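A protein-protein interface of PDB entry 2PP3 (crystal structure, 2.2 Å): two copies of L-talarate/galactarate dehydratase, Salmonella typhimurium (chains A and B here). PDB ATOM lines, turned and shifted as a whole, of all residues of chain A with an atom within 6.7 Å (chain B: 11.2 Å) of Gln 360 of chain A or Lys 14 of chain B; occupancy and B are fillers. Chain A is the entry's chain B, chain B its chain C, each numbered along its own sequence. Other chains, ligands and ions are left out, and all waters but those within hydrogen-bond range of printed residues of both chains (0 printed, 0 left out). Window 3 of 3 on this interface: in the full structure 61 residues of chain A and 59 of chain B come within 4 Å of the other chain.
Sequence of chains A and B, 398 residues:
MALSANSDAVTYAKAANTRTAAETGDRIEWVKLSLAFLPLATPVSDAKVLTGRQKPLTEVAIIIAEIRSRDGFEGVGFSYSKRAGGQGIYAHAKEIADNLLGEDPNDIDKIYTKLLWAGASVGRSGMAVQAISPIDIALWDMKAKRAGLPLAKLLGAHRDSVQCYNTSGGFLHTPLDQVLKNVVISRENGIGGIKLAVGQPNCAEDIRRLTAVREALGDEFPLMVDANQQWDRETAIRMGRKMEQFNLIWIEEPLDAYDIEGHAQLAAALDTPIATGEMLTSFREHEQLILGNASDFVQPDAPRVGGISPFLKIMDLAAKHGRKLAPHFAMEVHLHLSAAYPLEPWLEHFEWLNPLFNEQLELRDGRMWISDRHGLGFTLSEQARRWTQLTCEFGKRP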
ATOM      1  N   ASN A 189      20.987   6.636   0.225  1.00  0.00           N
ATOM      2  CA  ASN A 189      20.573   7.594   1.244  1.00  0.00           C
ATOM      3  C   ASN A 189      19.272   7.193   1.930  1.00  0.00           C
ATOM      4  O   ASN A 189      18.751   7.932   2.763  1.00  0.00           O
ATOM      5  CB  ASN A 189      20.436   8.985   0.630  1.00  0.00           C
ATOM      6  CG  ASN A 189      21.777   9.630   0.357  1.00  0.00           C
ATOM      7  OD1 ASN A 189      22.468  10.062   1.281  1.00  0.00           O
ATOM      8  ND2 ASN A 189      22.160   9.688  -0.913  1.00  0.00           N
ATOM      9  N   MET A 331       7.747  19.196   0.558  1.00  0.00           N
ATOM     10  CA  MET A 331       7.725  18.181   1.604  1.00  0.00           C
ATOM     11  C   MET A 331       7.781  18.762   3.015  1.00  0.00           C
ATOM     12  O   MET A 331       7.317  18.130   3.964  1.00  0.00           O
ATOM     13  CB  MET A 331       8.864  17.174   1.407  1.00  0.00           C
ATOM     14  CG  MET A 331      10.238  17.789   1.255  1.00  0.00           C
ATOM     15  SD  MET A 331      11.518  16.520   1.097  1.00  0.00           S
ATOM     16  CE  MET A 331      12.741  17.152   2.259  1.00  0.00           C
ATOM     17  N   GLU A 332       8.337  19.962   3.150  1.00  0.00           N
ATOM     18  CA  GLU A 332       8.435  20.617   4.453  1.00  0.00           C
ATOM     19  C   GLU A 332       7.052  20.793   5.081  1.00  0.00           C
ATOM     20  O   GLU A 332       6.911  20.775   6.308  1.00  0.00           O
ATOM     21  CB  GLU A 332       9.107  21.990   4.324  1.00  0.00           C
ATOM     22  CG  GLU A 332      10.600  21.966   3.977  1.00  0.00           C
ATOM     23  CD  GLU A 332      10.899  21.361   2.608  1.00  0.00           C
ATOM     24  OE1 GLU A 332      10.067  21.507   1.683  1.00  0.00           O
ATOM     25  OE2 GLU A 332      11.984  20.754   2.454  1.00  0.00           O
ATOM     26  N   GLU A 351      15.580  18.288  -3.141  1.00  0.00           N
ATOM     27  CA  GLU A 351      16.570  18.858  -2.232  1.00  0.00           C
ATOM     28  C   GLU A 351      16.545  20.379  -2.385  1.00  0.00           C
ATOM     29  O   GLU A 351      17.023  21.115  -1.528  1.00  0.00           O
ATOM     30  CB  GLU A 351      17.971  18.331  -2.554  1.00  0.00           C
ATOM     31  CG  GLU A 351      18.448  18.632  -3.970  1.00  0.00           C
ATOM     32  CD  GLU A 351      18.092  17.537  -4.955  1.00  0.00           C
ATOM     33  OE1 GLU A 351      16.921  17.102  -4.976  1.00  0.00           O
ATOM     34  OE2 GLU A 351      18.987  17.113  -5.713  1.00  0.00           O
ATOM     35  N   LEU A 353      14.701  22.924  -1.798  1.00  0.00           N
ATOM     36  CA  LEU A 353      14.419  23.820  -0.683  1.00  0.00           C
ATOM     37  C   LEU A 353      15.253  23.633   0.584  1.00  0.00           C
ATOM     38  O   LEU A 353      15.144  24.440   1.507  1.00  0.00           O
ATOM     39  CB  LEU A 353      12.929  23.754  -0.316  1.00  0.00           C
ATOM     40  CG  LEU A 353      11.971  24.624  -1.140  1.00  0.00           C
ATOM     41  CD1 LEU A 353      12.007  24.215  -2.604  1.00  0.00           C
ATOM     42  CD2 LEU A 353      10.562  24.491  -0.588  1.00  0.00           C
ATOM     43  N   ASN A 354      16.082  22.593   0.637  1.00  0.00           N
ATOM     44  CA  ASN A 354      16.898  22.350   1.833  1.00  0.00           C
ATOM     45  C   ASN A 354      17.634  23.590   2.346  1.00  0.00           C
ATOM     46  O   ASN A 354      17.650  23.848   3.547  1.00  0.00           O
ATOM     47  CB  ASN A 354      17.922  21.229   1.590  1.00  0.00           C
ATOM     48  CG  ASN A 354      17.273  19.875   1.381  1.00  0.00           C
ATOM     49  OD1 ASN A 354      16.174  19.617   1.870  1.00  0.00           O
ATOM     50  ND2 ASN A 354      17.961  18.992   0.667  1.00  0.00           N
ATOM     51  N   PRO A 355      18.252  24.374   1.444  1.00  0.00           N
ATOM     52  CA  PRO A 355      18.979  25.577   1.867  1.00  0.00           C
ATOM     53  C   PRO A 355      18.144  26.740   2.408  1.00  0.00           C
ATOM     54  O   PRO A 355      18.693  27.714   2.919  1.00  0.00           O
ATOM     55  CB  PRO A 355      19.777  25.955   0.618  1.00  0.00           C
ATOM     56  CG  PRO A 355      18.930  25.445  -0.496  1.00  0.00           C
ATOM     57  CD  PRO A 355      18.481  24.103   0.013  1.00  0.00           C
ATOM     58  N   LEU A 356      16.825  26.658   2.299  1.00  0.00           N
ATOM     59  CA  LEU A 356      15.982  27.736   2.813  1.00  0.00           C
ATOM     60  C   LEU A 356      15.854  27.654   4.332  1.00  0.00           C
ATOM     61  O   LEU A 356      15.586  28.654   5.000  1.00  0.00           O
ATOM     62  CB  LEU A 356      14.576  27.663   2.214  1.00  0.00           C
ATOM     63  CG  LEU A 356      14.417  28.005   0.737  1.00  0.00           C
ATOM     64  CD1 LEU A 356      12.941  27.993   0.386  1.00  0.00           C
ATOM     65  CD2 LEU A 356      15.023  29.377   0.459  1.00  0.00           C
ATOM     66  N   PHE A 357      16.052  26.454   4.868  1.00  0.00           N
ATOM     67  CA  PHE A 357      15.900  26.230   6.298  1.00  0.00           C
ATOM     68  C   PHE A 357      17.152  25.731   7.000  1.00  0.00           C
ATOM     69  O   PHE A 357      18.010  25.093   6.395  1.00  0.00           O
ATOM     70  CB  PHE A 357      14.763  25.233   6.521  1.00  0.00           C
ATOM     71  CG  PHE A 357      13.553  25.502   5.672  1.00  0.00           C
ATOM     72  CD1 PHE A 357      12.748  26.609   5.915  1.00  0.00           C
ATOM     73  CD2 PHE A 357      13.237  24.664   4.609  1.00  0.00           C
ATOM     74  CE1 PHE A 357      11.642  26.878   5.110  1.00  0.00           C
ATOM     75  CE2 PHE A 357      12.137  24.924   3.798  1.00  0.00           C
ATOM     76  CZ  PHE A 357      11.338  26.031   4.049  1.00  0.00           C
ATOM     77  N   ASN A 358      17.231  26.021   8.293  1.00  0.00           N
ATOM     78  CA  ASN A 358      18.357  25.608   9.122  1.00  0.00           C
ATOM     79  C   ASN A 358      18.280  24.119   9.458  1.00  0.00           C
ATOM     80  O   ASN A 358      19.306  23.458   9.617  1.00  0.00           O
ATOM     81  CB  ASN A 358      18.361  26.420  10.416  1.00  0.00           C
ATOM     82  CG  ASN A 358      18.633  27.889  10.177  1.00  0.00           C
ATOM     83  OD1 ASN A 358      17.991  28.756  10.768  1.00  0.00           O
ATOM     84  ND2 ASN A 358      19.599  28.175   9.314  1.00  0.00           N
ATOM     85  N   GLU A 359      17.059  23.599   9.556  1.00  0.00           N
ATOM     86  CA  GLU A 359      16.839  22.195   9.888  1.00  0.00           C
ATOM     87  C   GLU A 359      16.593  21.339   8.645  1.00  0.00           C
ATOM     88  O   GLU A 359      16.090  21.827   7.637  1.00  0.00           O
ATOM     89  CB  GLU A 359      15.633  22.061  10.828  1.00  0.00           C
ATOM     90  CG  GLU A 359      15.621  23.022  12.018  1.00  0.00           C
ATOM     91  CD  GLU A 359      15.174  24.438  11.656  1.00  0.00           C
ATOM     92  OE1 GLU A 359      14.859  24.699  10.475  1.00  0.00           O
ATOM     93  OE2 GLU A 359      15.132  25.297  12.564  1.00  0.00           O
ATOM     94  N   GLN A 360      16.944  20.061   8.731  1.00  0.00           N
ATOM     95  CA  GLN A 360      16.750  19.124   7.629  1.00  0.00           C
ATOM     96  C   GLN A 360      15.957  17.911   8.119  1.00  0.00           C
ATOM     97  O   GLN A 360      16.129  17.466   9.255  1.00  0.00           O
ATOM     98  CB  GLN A 360      18.104  18.669   7.076  1.00  0.00           C
ATOM     99  CG  GLN A 360      18.997  19.816   6.619  1.00  0.00           C
ATOM    100  CD  GLN A 360      18.385  20.625   5.484  1.00  0.00           C
ATOM    101  OE1 GLN A 360      18.692  21.805   5.314  1.00  0.00           O
ATOM    102  NE2 GLN A 360      17.523  19.988   4.696  1.00  0.00           N
ATOM    103  N   LEU A 361      15.083  17.380   7.269  1.00  0.00           N
ATOM    104  CA  LEU A 361      14.283  16.216   7.639  1.00  0.00           C
ATOM    105  C   LEU A 361      15.118  14.937   7.625  1.00  0.00           C
ATOM    106  O   LEU A 361      16.048  14.793   6.836  1.00  0.00           O
ATOM    107  CB  LEU A 361      13.084  16.066   6.698  1.00  0.00           C
ATOM    108  CG  LEU A 361      11.994  17.141   6.790  1.00  0.00           C
ATOM    109  CD1 LEU A 361      10.935  16.880   5.732  1.00  0.00           C
ATOM    110  CD2 LEU A 361      11.370  17.139   8.184  1.00  0.00           C
ATOM    111  N   GLU A 362      14.778  14.011   8.510  1.00  0.00           N
ATOM    112  CA  GLU A 362      15.492  12.750   8.602  1.00  0.00           C
ATOM    113  C   GLU A 362      14.899  11.705   7.656  1.00  0.00           C
ATOM    114  O   GLU A 362      13.714  11.380   7.738  1.00  0.00           O
ATOM    115  CB  GLU A 362      15.442  12.242  10.045  1.00  0.00           C
ATOM    116  CG  GLU A 362      16.098  10.889  10.261  1.00  0.00           C
ATOM    117  CD  GLU A 362      15.874  10.346  11.668  1.00  0.00           C
ATOM    118  OE1 GLU A 362      16.307   9.205  11.939  1.00  0.00           O
ATOM    119  OE2 GLU A 362      15.264  11.055  12.500  1.00  0.00           O
ATOM    120  N   LEU A 363      15.734  11.192   6.756  1.00  0.00           N
ATOM    121  CA  LEU A 363      15.326  10.172   5.794  1.00  0.00           C
ATOM    122  C   LEU A 363      16.002   8.860   6.166  1.00  0.00           C
ATOM    123  O   LEU A 363      17.225   8.754   6.121  1.00  0.00           O
ATOM    124  CB  LEU A 363      15.745  10.567   4.374  1.00  0.00           C
ATOM    125  CG  LEU A 363      15.457   9.511   3.298  1.00  0.00           C
ATOM    126  CD1 LEU A 363      13.961   9.269   3.223  1.00  0.00           C
ATOM    127  CD2 LEU A 363      15.985   9.976   1.944  1.00  0.00           C
ATOM    128  N   SER A 371      10.050  15.189  12.946  1.00  0.00           N
ATOM    129  CA  SER A 371      10.892  15.518  14.089  1.00  0.00           C
ATOM    130  C   SER A 371      10.039  16.045  15.242  1.00  0.00           C
ATOM    131  O   SER A 371       8.844  16.292  15.081  1.00  0.00           O
ATOM    132  CB  SER A 371      11.950  16.559  13.705  1.00  0.00           C
ATOM    133  OG  SER A 371      11.442  17.878  13.800  1.00  0.00           O
ATOM    134  N   ARG A 373      10.354  18.894  16.578  1.00  0.00           N
ATOM    135  CA  ARG A 373      10.235  20.350  16.481  1.00  0.00           C
ATOM    136  C   ARG A 373       8.768  20.755  16.319  1.00  0.00           C
ATOM    137  O   ARG A 373       8.002  20.053  15.669  1.00  0.00           O
ATOM    138  CB  ARG A 373      11.072  20.864  15.305  1.00  0.00           C
ATOM    139  CG  ARG A 373      12.572  20.582  15.449  1.00  0.00           C
ATOM    140  CD  ARG A 373      13.397  21.278  14.365  1.00  0.00           C
ATOM    141  NE  ARG A 373      13.164  20.712  13.038  1.00  0.00           N
ATOM    142  CZ  ARG A 373      13.727  19.595  12.587  1.00  0.00           C
ATOM    143  NH1 ARG A 373      14.571  18.916  13.354  1.00  0.00           N
ATOM    144  NH2 ARG A 373      13.436  19.151  11.372  1.00  0.00           N
ATOM    145  N   GLY A 377       8.374  22.971  11.982  1.00  0.00           N
ATOM    146  CA  GLY A 377       9.679  22.479  12.391  1.00  0.00           C
ATOM    147  C   GLY A 377      10.825  23.023  11.561  1.00  0.00           C
ATOM    148  O   GLY A 377      11.855  22.362  11.394  1.00  0.00           O
ATOM    149  N   PHE A 378      10.658  24.233  11.039  1.00  0.00           N
ATOM    150  CA  PHE A 378      11.691  24.850  10.219  1.00  0.00           C
ATOM    151  C   PHE A 378      11.828  26.322  10.530  1.00  0.00           C
ATOM    152  O   PHE A 378      10.836  26.994  10.809  1.00  0.00           O
ATOM    153  CB  PHE A 378      11.355  24.705   8.727  1.00  0.00           C
ATOM    154  CG  PHE A 378      11.481  23.301   8.201  1.00  0.00           C
ATOM    155  CD1 PHE A 378      12.734  22.732   7.985  1.00  0.00           C
ATOM    156  CD2 PHE A 378      10.347  22.550   7.909  1.00  0.00           C
ATOM    157  CE1 PHE A 378      12.856  21.436   7.484  1.00  0.00           C
ATOM    158  CE2 PHE A 378      10.457  21.252   7.407  1.00  0.00           C
ATOM    159  CZ  PHE A 378      11.716  20.693   7.194  1.00  0.00           C
ATOM    160  N   SER B   4      23.454  27.616  -5.641  1.00  0.00           N
ATOM    161  CA  SER B   4      22.633  26.645  -6.428  1.00  0.00           C
ATOM    162  C   SER B   4      21.875  25.661  -5.541  1.00  0.00           C
ATOM    163  O   SER B   4      22.443  25.064  -4.624  1.00  0.00           O
ATOM    164  CB  SER B   4      23.520  25.858  -7.391  1.00  0.00           C
ATOM    165  OG  SER B   4      22.765  24.872  -8.079  1.00  0.00           O
ATOM    166  N   ALA B   5      20.591  25.484  -5.830  1.00  0.00           N
ATOM    167  CA  ALA B   5      19.761  24.574  -5.056  1.00  0.00           C
ATOM    168  C   ALA B   5      19.781  23.163  -5.634  1.00  0.00           C
ATOM    169  O   ALA B   5      19.241  22.237  -5.032  1.00  0.00           O
ATOM    170  CB  ALA B   5      18.328  25.098  -4.995  1.00  0.00           C
ATOM    171  N   THR B  11      21.515  15.184  -4.479  1.00  0.00           N
ATOM    172  CA  THR B  11      22.247  15.269  -3.223  1.00  0.00           C
ATOM    173  C   THR B  11      21.262  15.243  -2.057  1.00  0.00           C
ATOM    174  O   THR B  11      20.160  15.792  -2.144  1.00  0.00           O
ATOM    175  CB  THR B  11      23.098  16.558  -3.143  1.00  0.00           C
ATOM    176  OG1 THR B  11      22.242  17.704  -3.188  1.00  0.00           O
ATOM    177  CG2 THR B  11      24.079  16.624  -4.302  1.00  0.00           C
ATOM    178  N   TYR B  12      21.662  14.593  -0.969  1.00  0.00           N
ATOM    179  CA  TYR B  12      20.824  14.478   0.221  1.00  0.00           C
ATOM    180  C   TYR B  12      21.475  15.155   1.414  1.00  0.00           C
ATOM    181  O   TYR B  12      22.675  15.017   1.641  1.00  0.00           O
ATOM    182  CB  TYR B  12      20.563  13.005   0.533  1.00  0.00           C
ATOM    183  CG  TYR B  12      19.551  12.379  -0.394  1.00  0.00           C
ATOM    184  CD1 TYR B  12      18.190  12.437  -0.106  1.00  0.00           C
ATOM    185  CD2 TYR B  12      19.949  11.771  -1.584  1.00  0.00           C
ATOM    186  CE1 TYR B  12      17.246  11.908  -0.980  1.00  0.00           C
ATOM    187  CE2 TYR B  12      19.010  11.240  -2.469  1.00  0.00           C
ATOM    188  CZ  TYR B  12      17.660  11.313  -2.158  1.00  0.00           C
ATOM    189  OH  TYR B  12      16.725  10.798  -3.023  1.00  0.00           O
ATOM    190  N   ALA B  13      20.670  15.886   2.178  1.00  0.00           N
ATOM    191  CA  ALA B  13      21.161  16.602   3.348  1.00  0.00           C
ATOM    192  C   ALA B  13      21.292  15.689   4.560  1.00  0.00           C
ATOM    193  O   ALA B  13      21.063  14.479   4.476  1.00  0.00           O
ATOM    194  CB  ALA B  13      20.224  17.770   3.673  1.00  0.00           C
ATOM    195  N   LYS B  14      21.673  16.283   5.686  1.00  0.00           N
ATOM    196  CA  LYS B  14      21.821  15.552   6.937  1.00  0.00           C
ATOM    197  C   LYS B  14      21.275  16.377   8.092  1.00  0.00           C
ATOM    198  O   LYS B  14      21.615  17.552   8.246  1.00  0.00           O
ATOM    199  CB  LYS B  14      23.291  15.209   7.196  1.00  0.00           C
ATOM    200  CG  LYS B  14      23.670  13.795   6.789  1.00  0.00           C
ATOM    201  CD  LYS B  14      22.818  12.766   7.529  1.00  0.00           C
ATOM    202  CE  LYS B  14      23.286  11.345   7.246  1.00  0.00           C
ATOM    203  NZ  LYS B  14      23.283  11.031   5.791  1.00  0.00           N
ATOM    204  N   ALA B  15      20.420  15.754   8.897  1.00  0.00           N
ATOM    205  CA  ALA B  15      19.819  16.426  10.041  1.00  0.00           C
ATOM    206  C   ALA B  15      20.631  16.178  11.310  1.00  0.00           C
ATOM    207  O   ALA B  15      21.363  15.188  11.408  1.00  0.00           O
ATOM    208  CB  ALA B  15      18.388  15.937  10.234  1.00  0.00           C
ATOM    209  N   ALA B  16      20.498  17.084  12.274  1.00  0.00           N
ATOM    210  CA  ALA B  16      21.206  16.966  13.546  1.00  0.00           C
ATOM    211  C   ALA B  16      20.242  16.452  14.612  1.00  0.00           C
ATOM    212  O   ALA B  16      20.435  15.365  15.160  1.00  0.00           O
ATOM    213  CB  ALA B  16      21.778  18.324  13.959  1.00  0.00           C
ATOM    214  N   ASN B  17      19.204  17.242  14.894  1.00  0.00           N
ATOM    215  CA  ASN B  17      18.188  16.878  15.883  1.00  0.00           C
ATOM    216  C   ASN B  17      17.516  15.585  15.418  1.00  0.00           C
ATOM    217  O   ASN B  17      16.568  15.612  14.625  1.00  0.00           O
ATOM    218  CB  ASN B  17      17.140  17.993  16.001  1.00  0.00           C
ATOM    219  CG  ASN B  17      16.151  17.757  17.137  1.00  0.00           C
ATOM    220  OD1 ASN B  17      15.589  16.668  17.272  1.00  0.00           O
ATOM    221  ND2 ASN B  17      15.927  18.784  17.952  1.00  0.00           N
ATOM    222  N   THR B  18      18.009  14.455  15.917  1.00  0.00           N
ATOM    223  CA  THR B  18      17.469  13.158  15.531  1.00  0.00           C
ATOM    224  C   THR B  18      16.251  12.766  16.377  1.00  0.00           C
ATOM    225  O   THR B  18      15.765  11.638  16.285  1.00  0.00           O
ATOM    226  CB  THR B  18      18.557  12.049  15.643  1.00  0.00           C
ATOM    227  OG1 THR B  18      19.821  12.564  15.197  1.00  0.00           O
ATOM    228  CG2 THR B  18      18.189  10.850  14.769  1.00  0.00           C
ATOM    229  N   ARG B  19      15.756  13.696  17.193  1.00  0.00           N
ATOM    230  CA  ARG B  19      14.594  13.418  18.035  1.00  0.00           C
ATOM    231  C   ARG B  19      13.318  13.429  17.198  1.00  0.00           C
ATOM    232  O   ARG B  19      13.039  14.395  16.482  1.00  0.00           O
ATOM    233  CB  ARG B  19      14.481  14.448  19.161  1.00  0.00           C
ATOM    234  CG  ARG B  19      15.752  14.602  19.977  1.00  0.00           C
ATOM    235  CD  ARG B  19      15.513  15.422  21.235  1.00  0.00           C
ATOM    236  NE  ARG B  19      14.538  14.782  22.112  1.00  0.00           N
ATOM    237  CZ  ARG B  19      14.616  13.519  22.520  1.00  0.00           C
ATOM    238  NH1 ARG B  19      15.625  12.749  22.132  1.00  0.00           N
ATOM    239  NH2 ARG B  19      13.686  13.021  23.323  1.00  0.00           N
ATOM    240  N   THR B  20      12.546  12.352  17.302  1.00  0.00           N
ATOM    241  CA  THR B  20      11.309  12.200  16.545  1.00  0.00           C
ATOM    242  C   THR B  20      10.079  12.522  17.376  1.00  0.00           C
ATOM    243  O   THR B  20      10.096  12.391  18.603  1.00  0.00           O
ATOM    244  CB  THR B  20      11.164  10.763  16.023  1.00  0.00           C
ATOM    245  OG1 THR B  20      11.046   9.864  17.132  1.00  0.00           O
ATOM    246  CG2 THR B  20      12.381  10.376  15.196  1.00  0.00           C
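O of Glu 351 of chain A sits close to ND2 of Asn 354 of chain A (3.2 Å). The side-chain hydroxyl of Thr 18 of chain B sits at hydrogen-bond distance from the backbone carbonyl oxygen of Ala 16 of chain B, 2.9 Å away. N of Arg 19 of chain B is in hydrogen-bond range of OD1 of Asn 17 of chain B, at 3.0 Å. The backbone NH (N) of Arg 373 of chain A lies close to the side-chain hydroxyl (OG) of Ser 371 of chain A (3.2 Å). The backbone carbonyl oxygen of Asn 354 of chain A lies close to the side-chain amide oxygen of Gln 360 of chain A, 2.9 Å away. The guanidinium group (NE) of Arg 373 of chain A is in hydrogen-bond range of the backbone carbonyl oxygen (O) of Gly 377 of chain A.
Gln 360 of chain A touches just these residues of chain B: Ala 13, Lys 14 and Ala 15. Lys 14 of chain B touches just one residue of chain A: Gln 360. No residue of chain B comes within 4 Å of Pro 355 of chain A. No residue of chain B comes within 4 Å of Leu 361 of chain A. Printed residues of chain A within 4 Å of Asn 17 of chain B: Arg 373. Of the printed residues of chain B, Arg 373 of chain A touches Asn 17 (3.8 Å). Leu 353 of chain A touches none of the printed residues of chain B. The nearest residue of chain A that does not touch Lys 14 of chain B is Asn 189 of chain A (4.7 Å). The nearest printed residue of chain B that does not touch Arg 373 of chain A is Arg 19 of chain B (5.2 Å).
No position is printed for both chains. Of the 11 pairs that touch across the chains among the printed residues, none has its exchanged pair printed and touching as well.
Of the 12 printed residues of chain B, 9 touch a printed residue of chain A. Printed residues of chain B that touch a printed residue of chain A: Ala 5, Thr 11, Tyr 12, Ala 13, Lys 14, Ala 15, Asn 17, Thr 18 and Arg 19. Hydrophobic or aromatic side chains of chain B within 4 Å of the printed part of chain A: Tyr 12, Ala 13 and Ala 15. Among the printed residues, 11 pairs touch across the chains. Among the printed residues, no Asp or Glu carboxylate lies within 4 Å of a Lys or Arg side-chain nitrogen of the other chain.
OE2 of Glu 351 of chain A is in hydrogen-bond range of N of Thr 11 of chain B (3.4 Å).
Asn 189 of chain A touches Tyr 12 of chain B (ND2 to CD2, 3.1 Å). CG of Glu 351 of chain A touches O of Ala 5 of chain B, at 3.8 Å. Asn 354 of chain A touches Ala 13 of chain B (ND2 to CB, 3.96 Å). Ala 13 of chain B touches Gln 360 of chain A. Lys 14 of chain B touches Gln 360 of chain A (O to CG, 3.8 Å). O of Gln 360 of chain A touches CB of Ala 15 of chain B (2.9 Å). Glu 362 of chain A touches Thr 18 of chain B. Leu 363 of chain A touches Tyr 12 of chain B. CA of Ser 371 of chain A touches O of Arg 19 of chain B, 3.4 Å away. Arg 373 of chain A touches Asn 17 of chain B (NH1 to CB, 3.8 Å).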
